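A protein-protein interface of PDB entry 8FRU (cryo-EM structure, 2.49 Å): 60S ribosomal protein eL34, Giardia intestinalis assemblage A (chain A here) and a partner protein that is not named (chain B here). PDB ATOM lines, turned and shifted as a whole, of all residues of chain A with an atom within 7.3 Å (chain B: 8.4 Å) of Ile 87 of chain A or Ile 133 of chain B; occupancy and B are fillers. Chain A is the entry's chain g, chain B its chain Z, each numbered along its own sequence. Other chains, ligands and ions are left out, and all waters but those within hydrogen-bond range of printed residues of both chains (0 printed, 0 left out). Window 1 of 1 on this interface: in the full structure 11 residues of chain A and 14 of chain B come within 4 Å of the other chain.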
ATOM      1  N   PRO A  73      15.757  30.905  16.621  1.00  0.00           N
ATOM      2  CA  PRO A  73      15.904  29.494  16.237  1.00  0.00           C
ATOM      3  C   PRO A  73      15.650  29.195  14.767  1.00  0.00           C
ATOM      4  O   PRO A  73      16.368  28.369  14.198  1.00  0.00           O
ATOM      5  CB  PRO A  73      14.895  28.804  17.153  1.00  0.00           C
ATOM      6  CG  PRO A  73      14.962  29.617  18.385  1.00  0.00           C
ATOM      7  CD  PRO A  73      15.086  31.042  17.921  1.00  0.00           C
ATOM      8  N   TYR A  74      14.672  29.818  14.120  1.00  0.00           N
ATOM      9  CA  TYR A  74      14.468  29.591  12.693  1.00  0.00           C
ATOM     10  C   TYR A  74      14.785  30.832  11.868  1.00  0.00           C
ATOM     11  O   TYR A  74      14.243  31.017  10.780  1.00  0.00           O
ATOM     12  CB  TYR A  74      13.043  29.120  12.416  1.00  0.00           C
ATOM     13  CG  TYR A  74      12.872  27.626  12.509  1.00  0.00           C
ATOM     14  CD1 TYR A  74      12.839  26.991  13.738  1.00  0.00           C
ATOM     15  CD2 TYR A  74      12.746  26.852  11.372  1.00  0.00           C
ATOM     16  CE1 TYR A  74      12.684  25.633  13.830  1.00  0.00           C
ATOM     17  CE2 TYR A  74      12.589  25.492  11.455  1.00  0.00           C
ATOM     18  CZ  TYR A  74      12.560  24.887  12.685  1.00  0.00           C
ATOM     19  OH  TYR A  74      12.407  23.528  12.773  1.00  0.00           O
ATOM     20  N   LEU A  78      11.613  31.792   8.556  1.00  0.00           N
ATOM     21  CA  LEU A  78      10.252  32.237   8.797  1.00  0.00           C
ATOM     22  C   LEU A  78      10.254  33.407   9.767  1.00  0.00           C
ATOM     23  O   LEU A  78      11.229  33.654  10.479  1.00  0.00           O
ATOM     24  CB  LEU A  78       9.368  31.102   9.317  1.00  0.00           C
ATOM     25  CG  LEU A  78       9.763  30.384  10.595  1.00  0.00           C
ATOM     26  CD1 LEU A  78       9.049  31.000  11.760  1.00  0.00           C
ATOM     27  CD2 LEU A  78       9.408  28.917  10.475  1.00  0.00           C
ATOM     28  N   GLY A  80       8.689  35.927  12.917  1.00  0.00           N
ATOM     29  CA  GLY A  80       8.362  35.678  14.309  1.00  0.00           C
ATOM     30  C   GLY A  80       6.935  35.203  14.504  1.00  0.00           C
ATOM     31  O   GLY A  80       6.666  34.358  15.359  1.00  0.00           O
ATOM     32  N   ALA A  82       5.088  33.448  12.372  1.00  0.00           N
ATOM     33  CA  ALA A  82       4.942  32.070  11.918  1.00  0.00           C
ATOM     34  C   ALA A  82       5.587  31.088  12.882  1.00  0.00           C
ATOM     35  O   ALA A  82       5.161  29.932  12.962  1.00  0.00           O
ATOM     36  CB  ALA A  82       5.537  31.911  10.520  1.00  0.00           C
ATOM     37  N   LEU A  83       6.620  31.517  13.607  1.00  0.00           N
ATOM     38  CA  LEU A  83       7.273  30.628  14.558  1.00  0.00           C
ATOM     39  C   LEU A  83       6.387  30.361  15.767  1.00  0.00           C
ATOM     40  O   LEU A  83       6.371  29.244  16.296  1.00  0.00           O
ATOM     41  CB  LEU A  83       8.616  31.216  14.983  1.00  0.00           C
ATOM     42  CG  LEU A  83       9.480  30.358  15.904  1.00  0.00           C
ATOM     43  CD1 LEU A  83      10.043  29.158  15.171  1.00  0.00           C
ATOM     44  CD2 LEU A  83      10.589  31.190  16.486  1.00  0.00           C
ATOM     45  N   ARG A  84       5.636  31.367  16.216  1.00  0.00           N
ATOM     46  CA  ARG A  84       4.742  31.164  17.350  1.00  0.00           C
ATOM     47  C   ARG A  84       3.706  30.092  17.051  1.00  0.00           C
ATOM     48  O   ARG A  84       3.433  29.233  17.894  1.00  0.00           O
ATOM     49  CB  ARG A  84       4.048  32.470  17.718  1.00  0.00           C
ATOM     50  CG  ARG A  84       4.778  33.295  18.744  1.00  0.00           C
ATOM     51  CD  ARG A  84       3.875  34.383  19.280  1.00  0.00           C
ATOM     52  NE  ARG A  84       2.474  33.992  19.218  1.00  0.00           N
ATOM     53  CZ  ARG A  84       1.622  34.089  20.227  1.00  0.00           C
ATOM     54  NH1 ARG A  84       1.999  34.551  21.407  1.00  0.00           N
ATOM     55  NH2 ARG A  84       0.360  33.714  20.051  1.00  0.00           N
ATOM     56  N   ALA A  85       3.118  30.128  15.858  1.00  0.00           N
ATOM     57  CA  ALA A  85       2.081  29.162  15.521  1.00  0.00           C
ATOM     58  C   ALA A  85       2.620  27.738  15.552  1.00  0.00           C
ATOM     59  O   ALA A  85       1.949  26.821  16.036  1.00  0.00           O
ATOM     60  CB  ALA A  85       1.496  29.488  14.150  1.00  0.00           C
ATOM     61  N   HIS A  86       3.825  27.533  15.031  1.00  0.00           N
ATOM     62  CA  HIS A  86       4.415  26.202  15.045  1.00  0.00           C
ATOM     63  C   HIS A  86       4.699  25.734  16.465  1.00  0.00           C
ATOM     64  O   HIS A  86       4.498  24.559  16.787  1.00  0.00           O
ATOM     65  CB  HIS A  86       5.688  26.196  14.209  1.00  0.00           C
ATOM     66  CG  HIS A  86       5.438  26.110  12.738  1.00  0.00           C
ATOM     67  ND1 HIS A  86       5.115  27.210  11.974  1.00  0.00           N
ATOM     68  CD2 HIS A  86       5.468  25.058  11.888  1.00  0.00           C
ATOM     69  CE1 HIS A  86       4.952  26.837  10.719  1.00  0.00           C
ATOM     70  NE2 HIS A  86       5.162  25.537  10.639  1.00  0.00           N
ATOM     71  N   ILE A  87       5.178  26.630  17.325  1.00  0.00           N
ATOM     72  CA  ILE A  87       5.434  26.260  18.713  1.00  0.00           C
ATOM     73  C   ILE A  87       4.127  25.949  19.428  1.00  0.00           C
ATOM     74  O   ILE A  87       4.000  24.924  20.104  1.00  0.00           O
ATOM     75  CB  ILE A  87       6.220  27.373  19.429  1.00  0.00           C
ATOM     76  CG1 ILE A  87       7.641  27.463  18.877  1.00  0.00           C
ATOM     77  CG2 ILE A  87       6.264  27.122  20.917  1.00  0.00           C
ATOM     78  CD1 ILE A  87       8.351  28.727  19.254  1.00  0.00           C
ATOM     79  N   LEU A  88       3.132  26.824  19.285  1.00  0.00           N
ATOM     80  CA  LEU A  88       1.839  26.577  19.912  1.00  0.00           C
ATOM     81  C   LEU A  88       1.196  25.313  19.367  1.00  0.00           C
ATOM     82  O   LEU A  88       0.652  24.506  20.127  1.00  0.00           O
ATOM     83  CB  LEU A  88       0.911  27.767  19.695  1.00  0.00           C
ATOM     84  CG  LEU A  88       1.171  29.022  20.517  1.00  0.00           C
ATOM     85  CD1 LEU A  88       0.205  30.104  20.109  1.00  0.00           C
ATOM     86  CD2 LEU A  88       1.039  28.721  21.985  1.00  0.00           C
ATOM     87  N   GLU A  89       1.245  25.125  18.052  1.00  0.00           N
ATOM     88  CA  GLU A  89       0.593  23.970  17.448  1.00  0.00           C
ATOM     89  C   GLU A  89       1.243  22.666  17.888  1.00  0.00           C
ATOM     90  O   GLU A  89       0.548  21.687  18.172  1.00  0.00           O
ATOM     91  CB  GLU A  89       0.616  24.100  15.927  1.00  0.00           C
ATOM     92  CG  GLU A  89      -0.499  23.366  15.227  1.00  0.00           C
ATOM     93  CD  GLU A  89       0.008  22.532  14.074  1.00  0.00           C
ATOM     94  OE1 GLU A  89       1.228  22.567  13.814  1.00  0.00           O
ATOM     95  OE2 GLU A  89      -0.807  21.837  13.431  1.00  0.00           O
ATOM     96  N   SER A  90       2.575  22.624  17.937  1.00  0.00           N
ATOM     97  CA  SER A  90       3.252  21.396  18.340  1.00  0.00           C
ATOM     98  C   SER A  90       2.995  21.075  19.804  1.00  0.00           C
ATOM     99  O   SER A  90       2.764  19.914  20.157  1.00  0.00           O
ATOM    100  CB  SER A  90       4.752  21.506  18.074  1.00  0.00           C
ATOM    101  OG  SER A  90       5.406  22.202  19.117  1.00  0.00           O
ATOM    102  N   PHE A  91       3.039  22.082  20.673  1.00  0.00           N
ATOM    103  CA  PHE A  91       2.820  21.826  22.091  1.00  0.00           C
ATOM    104  C   PHE A  91       1.389  21.379  22.358  1.00  0.00           C
ATOM    105  O   PHE A  91       1.161  20.355  23.007  1.00  0.00           O
ATOM    106  CB  PHE A  91       3.148  23.071  22.906  1.00  0.00           C
ATOM    107  CG  PHE A  91       2.569  23.049  24.281  1.00  0.00           C
ATOM    108  CD1 PHE A  91       2.989  22.115  25.207  1.00  0.00           C
ATOM    109  CD2 PHE A  91       1.584  23.947  24.645  1.00  0.00           C
ATOM    110  CE1 PHE A  91       2.451  22.091  26.471  1.00  0.00           C
ATOM    111  CE2 PHE A  91       1.042  23.923  25.907  1.00  0.00           C
ATOM    112  CZ  PHE A  91       1.477  22.994  26.821  1.00  0.00           C
ATOM    113  N   LEU A  92       0.409  22.134  21.859  1.00  0.00           N
ATOM    114  CA  LEU A  92      -0.984  21.787  22.118  1.00  0.00           C
ATOM    115  C   LEU A  92      -1.344  20.440  21.513  1.00  0.00           C
ATOM    116  O   LEU A  92      -2.196  19.728  22.050  1.00  0.00           O
ATOM    117  CB  LEU A  92      -1.913  22.871  21.577  1.00  0.00           C
ATOM    118  CG  LEU A  92      -1.877  24.235  22.266  1.00  0.00           C
ATOM    119  CD1 LEU A  92      -2.400  25.301  21.339  1.00  0.00           C
ATOM    120  CD2 LEU A  92      -2.672  24.218  23.558  1.00  0.00           C
ATOM    121  N   ASN A  93      -0.728  20.079  20.390  1.00  0.00           N
ATOM    122  CA  ASN A  93      -1.034  18.797  19.773  1.00  0.00           C
ATOM    123  C   ASN A  93      -0.405  17.647  20.544  1.00  0.00           C
ATOM    124  O   ASN A  93      -1.045  16.614  20.760  1.00  0.00           O
ATOM    125  CB  ASN A  93      -0.560  18.788  18.323  1.00  0.00           C
ATOM    126  CG  ASN A  93      -1.696  18.965  17.341  1.00  0.00           C
ATOM    127  OD1 ASN A  93      -2.716  18.283  17.424  1.00  0.00           O
ATOM    128  ND2 ASN A  93      -1.528  19.888  16.404  1.00  0.00           N
ATOM    129  N   ILE B  13       6.763  27.903  28.340  1.00  0.00           N
ATOM    130  CA  ILE B  13       7.531  27.777  27.107  1.00  0.00           C
ATOM    131  C   ILE B  13       7.721  29.168  26.523  1.00  0.00           C
ATOM    132  O   ILE B  13       6.773  29.955  26.464  1.00  0.00           O
ATOM    133  CB  ILE B  13       6.839  26.843  26.098  1.00  0.00           C
ATOM    134  CG1 ILE B  13       6.784  25.426  26.666  1.00  0.00           C
ATOM    135  CG2 ILE B  13       7.570  26.854  24.779  1.00  0.00           C
ATOM    136  CD1 ILE B  13       6.148  24.419  25.757  1.00  0.00           C
ATOM    137  N   VAL B  14       8.942  29.476  26.109  1.00  0.00           N
ATOM    138  CA  VAL B  14       9.247  30.779  25.532  1.00  0.00           C
ATOM    139  C   VAL B  14       8.746  30.818  24.096  1.00  0.00           C
ATOM    140  O   VAL B  14       9.063  29.938  23.289  1.00  0.00           O
ATOM    141  CB  VAL B  14      10.751  31.066  25.604  1.00  0.00           C
ATOM    142  CG1 VAL B  14      11.028  32.489  25.170  1.00  0.00           C
ATOM    143  CG2 VAL B  14      11.251  30.840  27.007  1.00  0.00           C
ATOM    144  N   LEU B  15       7.956  31.838  23.776  1.00  0.00           N
ATOM    145  CA  LEU B  15       7.378  31.980  22.452  1.00  0.00           C
ATOM    146  C   LEU B  15       8.076  33.027  21.603  1.00  0.00           C
ATOM    147  O   LEU B  15       7.846  33.071  20.392  1.00  0.00           O
ATOM    148  CB  LEU B  15       5.894  32.339  22.557  1.00  0.00           C
ATOM    149  CG  LEU B  15       5.013  31.422  23.398  1.00  0.00           C
ATOM    150  CD1 LEU B  15       3.623  32.013  23.522  1.00  0.00           C
ATOM    151  CD2 LEU B  15       4.960  30.034  22.789  1.00  0.00           C
ATOM    152  N   GLN B  16       8.925  33.861  22.194  1.00  0.00           N
ATOM    153  CA  GLN B  16       9.509  34.980  21.481  1.00  0.00           C
ATOM    154  C   GLN B  16      10.958  35.149  21.904  1.00  0.00           C
ATOM    155  O   GLN B  16      11.377  34.659  22.953  1.00  0.00           O
ATOM    156  CB  GLN B  16       8.713  36.257  21.743  1.00  0.00           C
ATOM    157  CG  GLN B  16       8.553  37.129  20.537  1.00  0.00           C
ATOM    158  CD  GLN B  16       7.181  37.745  20.454  1.00  0.00           C
ATOM    159  OE1 GLN B  16       6.176  37.041  20.457  1.00  0.00           O
ATOM    160  NE2 GLN B  16       7.131  39.069  20.371  1.00  0.00           N
ATOM    161  N   GLY B  17      11.722  35.844  21.072  1.00  0.00           N
ATOM    162  CA  GLY B  17      13.089  36.182  21.401  1.00  0.00           C
ATOM    163  C   GLY B  17      14.099  35.160  20.928  1.00  0.00           C
ATOM    164  O   GLY B  17      13.817  34.262  20.136  1.00  0.00           O
ATOM    165  N   HIS B  19      15.601  32.837  22.747  1.00  0.00           N
ATOM    166  CA  HIS B  19      15.405  31.526  23.349  1.00  0.00           C
ATOM    167  C   HIS B  19      14.009  30.969  23.095  1.00  0.00           C
ATOM    168  O   HIS B  19      13.513  30.165  23.884  1.00  0.00           O
ATOM    169  CB  HIS B  19      15.681  31.590  24.850  1.00  0.00           C
ATOM    170  CG  HIS B  19      16.998  32.210  25.194  1.00  0.00           C
ATOM    171  ND1 HIS B  19      18.201  31.593  24.931  1.00  0.00           N
ATOM    172  CD2 HIS B  19      17.301  33.392  25.778  1.00  0.00           C
ATOM    173  CE1 HIS B  19      19.188  32.368  25.340  1.00  0.00           C
ATOM    174  NE2 HIS B  19      18.670  33.467  25.854  1.00  0.00           N
ATOM    175  N   ALA B  20      13.366  31.378  22.008  1.00  0.00           N
ATOM    176  CA  ALA B  20      12.026  30.895  21.719  1.00  0.00           C
ATOM    177  C   ALA B  20      12.034  29.388  21.506  1.00  0.00           C
ATOM    178  O   ALA B  20      12.968  28.831  20.926  1.00  0.00           O
ATOM    179  CB  ALA B  20      11.461  31.598  20.488  1.00  0.00           C
ATOM    180  N   GLY B  21      10.985  28.726  21.986  1.00  0.00           N
ATOM    181  CA  GLY B  21      10.855  27.292  21.864  1.00  0.00           C
ATOM    182  C   GLY B  21      11.512  26.488  22.959  1.00  0.00           C
ATOM    183  O   GLY B  21      11.468  25.254  22.908  1.00  0.00           O
ATOM    184  N   LYS B  22      12.120  27.134  23.942  1.00  0.00           N
ATOM    185  CA  LYS B  22      12.747  26.449  25.060  1.00  0.00           C
ATOM    186  C   LYS B  22      11.865  26.536  26.297  1.00  0.00           C
ATOM    187  O   LYS B  22      11.026  27.428  26.429  1.00  0.00           O
ATOM    188  CB  LYS B  22      14.126  27.043  25.346  1.00  0.00           C
ATOM    189  CG  LYS B  22      14.973  27.205  24.108  1.00  0.00           C
ATOM    190  CD  LYS B  22      16.385  27.604  24.456  1.00  0.00           C
ATOM    191  CE  LYS B  22      17.266  27.610  23.223  1.00  0.00           C
ATOM    192  NZ  LYS B  22      18.190  28.770  23.207  1.00  0.00           N
ATOM    193  N   HIS B  77       4.675  36.610  26.503  1.00  0.00           N
ATOM    194  CA  HIS B  77       5.555  35.821  25.654  1.00  0.00           C
ATOM    195  C   HIS B  77       5.761  34.406  26.176  1.00  0.00           C
ATOM    196  O   HIS B  77       6.697  33.726  25.745  1.00  0.00           O
ATOM    197  CB  HIS B  77       6.904  36.522  25.499  1.00  0.00           C
ATOM    198  CG  HIS B  77       6.824  37.855  24.823  1.00  0.00           C
ATOM    199  ND1 HIS B  77       7.804  38.812  24.954  1.00  0.00           N
ATOM    200  CD2 HIS B  77       5.887  38.387  24.008  1.00  0.00           C
ATOM    201  CE1 HIS B  77       7.471  39.879  24.252  1.00  0.00           C
ATOM    202  NE2 HIS B  77       6.313  39.647  23.666  1.00  0.00           N
ATOM    203  N   MET B  79       3.984  30.490  27.463  1.00  0.00           N
ATOM    204  CA  MET B  79       2.886  29.524  27.411  1.00  0.00           C
ATOM    205  C   MET B  79       2.904  28.669  28.669  1.00  0.00           C
ATOM    206  O   MET B  79       3.703  27.722  28.766  1.00  0.00           O
ATOM    207  CB  MET B  79       2.997  28.645  26.168  1.00  0.00           C
ATOM    208  CG  MET B  79       1.681  28.053  25.694  1.00  0.00           C
ATOM    209  SD  MET B  79       0.246  29.084  26.028  1.00  0.00           S
ATOM    210  CE  MET B  79      -1.027  27.837  26.179  1.00  0.00           C
ATOM    211  N   LYS B 130      13.702  18.078  24.720  1.00  0.00           N
ATOM    212  CA  LYS B 130      13.503  19.025  23.635  1.00  0.00           C
ATOM    213  C   LYS B 130      12.090  18.899  23.083  1.00  0.00           C
ATOM    214  O   LYS B 130      11.572  17.793  22.916  1.00  0.00           O
ATOM    215  CB  LYS B 130      14.525  18.786  22.523  1.00  0.00           C
ATOM    216  CG  LYS B 130      14.932  20.029  21.764  1.00  0.00           C
ATOM    217  CD  LYS B 130      14.296  20.058  20.387  1.00  0.00           C
ATOM    218  CE  LYS B 130      15.163  19.356  19.359  1.00  0.00           C
ATOM    219  NZ  LYS B 130      14.472  19.231  18.046  1.00  0.00           N
ATOM    220  N   LEU B 131      11.466  20.042  22.805  1.00  0.00           N
ATOM    221  CA  LEU B 131      10.114  20.055  22.267  1.00  0.00           C
ATOM    222  C   LEU B 131      10.189  19.966  20.749  1.00  0.00           C
ATOM    223  O   LEU B 131      10.669  20.910  20.109  1.00  0.00           O
ATOM    224  CB  LEU B 131       9.381  21.318  22.693  1.00  0.00           C
ATOM    225  CG  LEU B 131       8.088  21.676  21.959  1.00  0.00           C
ATOM    226  CD1 LEU B 131       6.881  21.080  22.658  1.00  0.00           C
ATOM    227  CD2 LEU B 131       7.950  23.180  21.843  1.00  0.00           C
ATOM    228  N   PRO B 132       9.734  18.876  20.135  1.00  0.00           N
ATOM    229  CA  PRO B 132       9.841  18.760  18.678  1.00  0.00           C
ATOM    230  C   PRO B 132       8.997  19.809  17.974  1.00  0.00           C
ATOM    231  O   PRO B 132       7.866  20.094  18.372  1.00  0.00           O
ATOM    232  CB  PRO B 132       9.326  17.344  18.398  1.00  0.00           C
ATOM    233  CG  PRO B 132       8.433  17.037  19.536  1.00  0.00           C
ATOM    234  CD  PRO B 132       9.010  17.741  20.730  1.00  0.00           C
ATOM    235  N   ILE B 133       9.561  20.380  16.913  1.00  0.00           N
ATOM    236  CA  ILE B 133       8.894  21.393  16.108  1.00  0.00           C
ATOM    237  C   ILE B 133       9.072  21.017  14.645  1.00  0.00           C
ATOM    238  O   ILE B 133      10.193  20.740  14.206  1.00  0.00           O
ATOM    239  CB  ILE B 133       9.458  22.798  16.376  1.00  0.00           C
ATOM    240  CG1 ILE B 133       8.868  23.371  17.658  1.00  0.00           C
ATOM    241  CG2 ILE B 133       9.146  23.719  15.219  1.00  0.00           C
ATOM    242  CD1 ILE B 133       9.785  24.340  18.361  1.00  0.00           C
ATOM    243  N   ASP B 134       7.977  21.012  13.893  1.00  0.00           N
ATOM    244  CA  ASP B 134       8.034  20.567  12.509  1.00  0.00           C
ATOM    245  C   ASP B 134       7.743  21.717  11.555  1.00  0.00           C
ATOM    246  O   ASP B 134       6.753  21.690  10.815  1.00  0.00           O
ATOM    247  CB  ASP B 134       7.057  19.412  12.279  1.00  0.00           C
ATOM    248  CG  ASP B 134       7.506  18.128  12.949  1.00  0.00           C
ATOM    249  OD1 ASP B 134       8.687  18.041  13.346  1.00  0.00           O
ATOM    250  OD2 ASP B 134       6.678  17.201  13.086  1.00  0.00           O
ATOM    251  N   ALA B 135       8.602  22.728  11.563  1.00  0.00           N
ATOM    252  CA  ALA B 135       8.468  23.849  10.651  1.00  0.00           C
ATOM    253  C   ALA B 135       8.978  23.471   9.263  1.00  0.00           C
ATOM    254  O   ALA B 135      10.154  23.654   8.951  1.00  0.00           O
ATOM    255  CB  ALA B 135       9.217  25.058  11.183  1.00  0.00           C
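The side-chain hydroxyl (OG) of Ser 90 of chain A lies within hydrogen-bond range of the backbone carbonyl oxygen (O) of Pro 132 of chain B (3.3 Å).
The backbone NH of Met 79 of chain B is in hydrogen-bond range of the backbone carbonyl oxygen of Ile 13 of chain B (3.0 Å). O of Val 14 of chain B lies within hydrogen-bond range of N of Gly 21 of chain B, 2.6 Å away. O of His 77 of chain B lies within hydrogen-bond range of N of Leu 15 of chain B (3.0 Å). A ring nitrogen (NE2) of His 77 of chain B is in hydrogen-bond range of the side-chain amide nitrogen (NE2) of Gln 16 of chain B. ND1 of His 86 of chain A lies within hydrogen-bond range of O of Ala 82 of chain A (2.9 Å). O of His 86 of chain A lies close to OG of Ser 90 of chain A (3.4 Å).
CG of Pro 73 of chain A touches O of Ala 20 of chain B, 3.3 Å away. Ile 133 of chain B touches Tyr 74 of chain A. Tyr 74 of chain A touches Ala 135 of chain B (CE2 to CB, 3.4 Å). CB of Ala 135 of chain B touches CD2 of Leu 78 of chain A, 3.9 Å away. CG of Arg 84 of chain A touches O of Leu 15 of chain B (3.5 Å). Asp 134 of chain B touches His 86 of chain A. CD2 of His 86 of chain A touches CA of Ala 135 of chain B (3.5 Å). Ile 87 of chain A touches Gly 21 of chain B. Ser 90 of chain A touches Leu 131 of chain B (OG to CD2, 3.9 Å). Phe 91 of chain A touches Ile 13 of chain B.
Ile 87 of chain A touches just these residues of chain B: Leu 15, Gly 21 and Ile 133. Of the printed residues of chain A, Met 79 of chain B touches Leu 88. Of the printed residues of chain A, Asp 134 of chain B touches His 86 (3.8 Å). Of the printed residues of chain A, Leu 131 of chain B touches Ser 90. Of the printed residues of chain B, Leu 88 of chain A touches Met 79.
Printed residues of chain A that touch a printed residue of chain B: Pro 73, Tyr 74, Leu 78, Arg 84, His 86, Ile 87, Leu 88, Ser 90 and Phe 91. Among the printed residues, no Asp or Glu carboxylate lies within 4 Å of a Lys or Arg side-chain nitrogen of the other chain.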
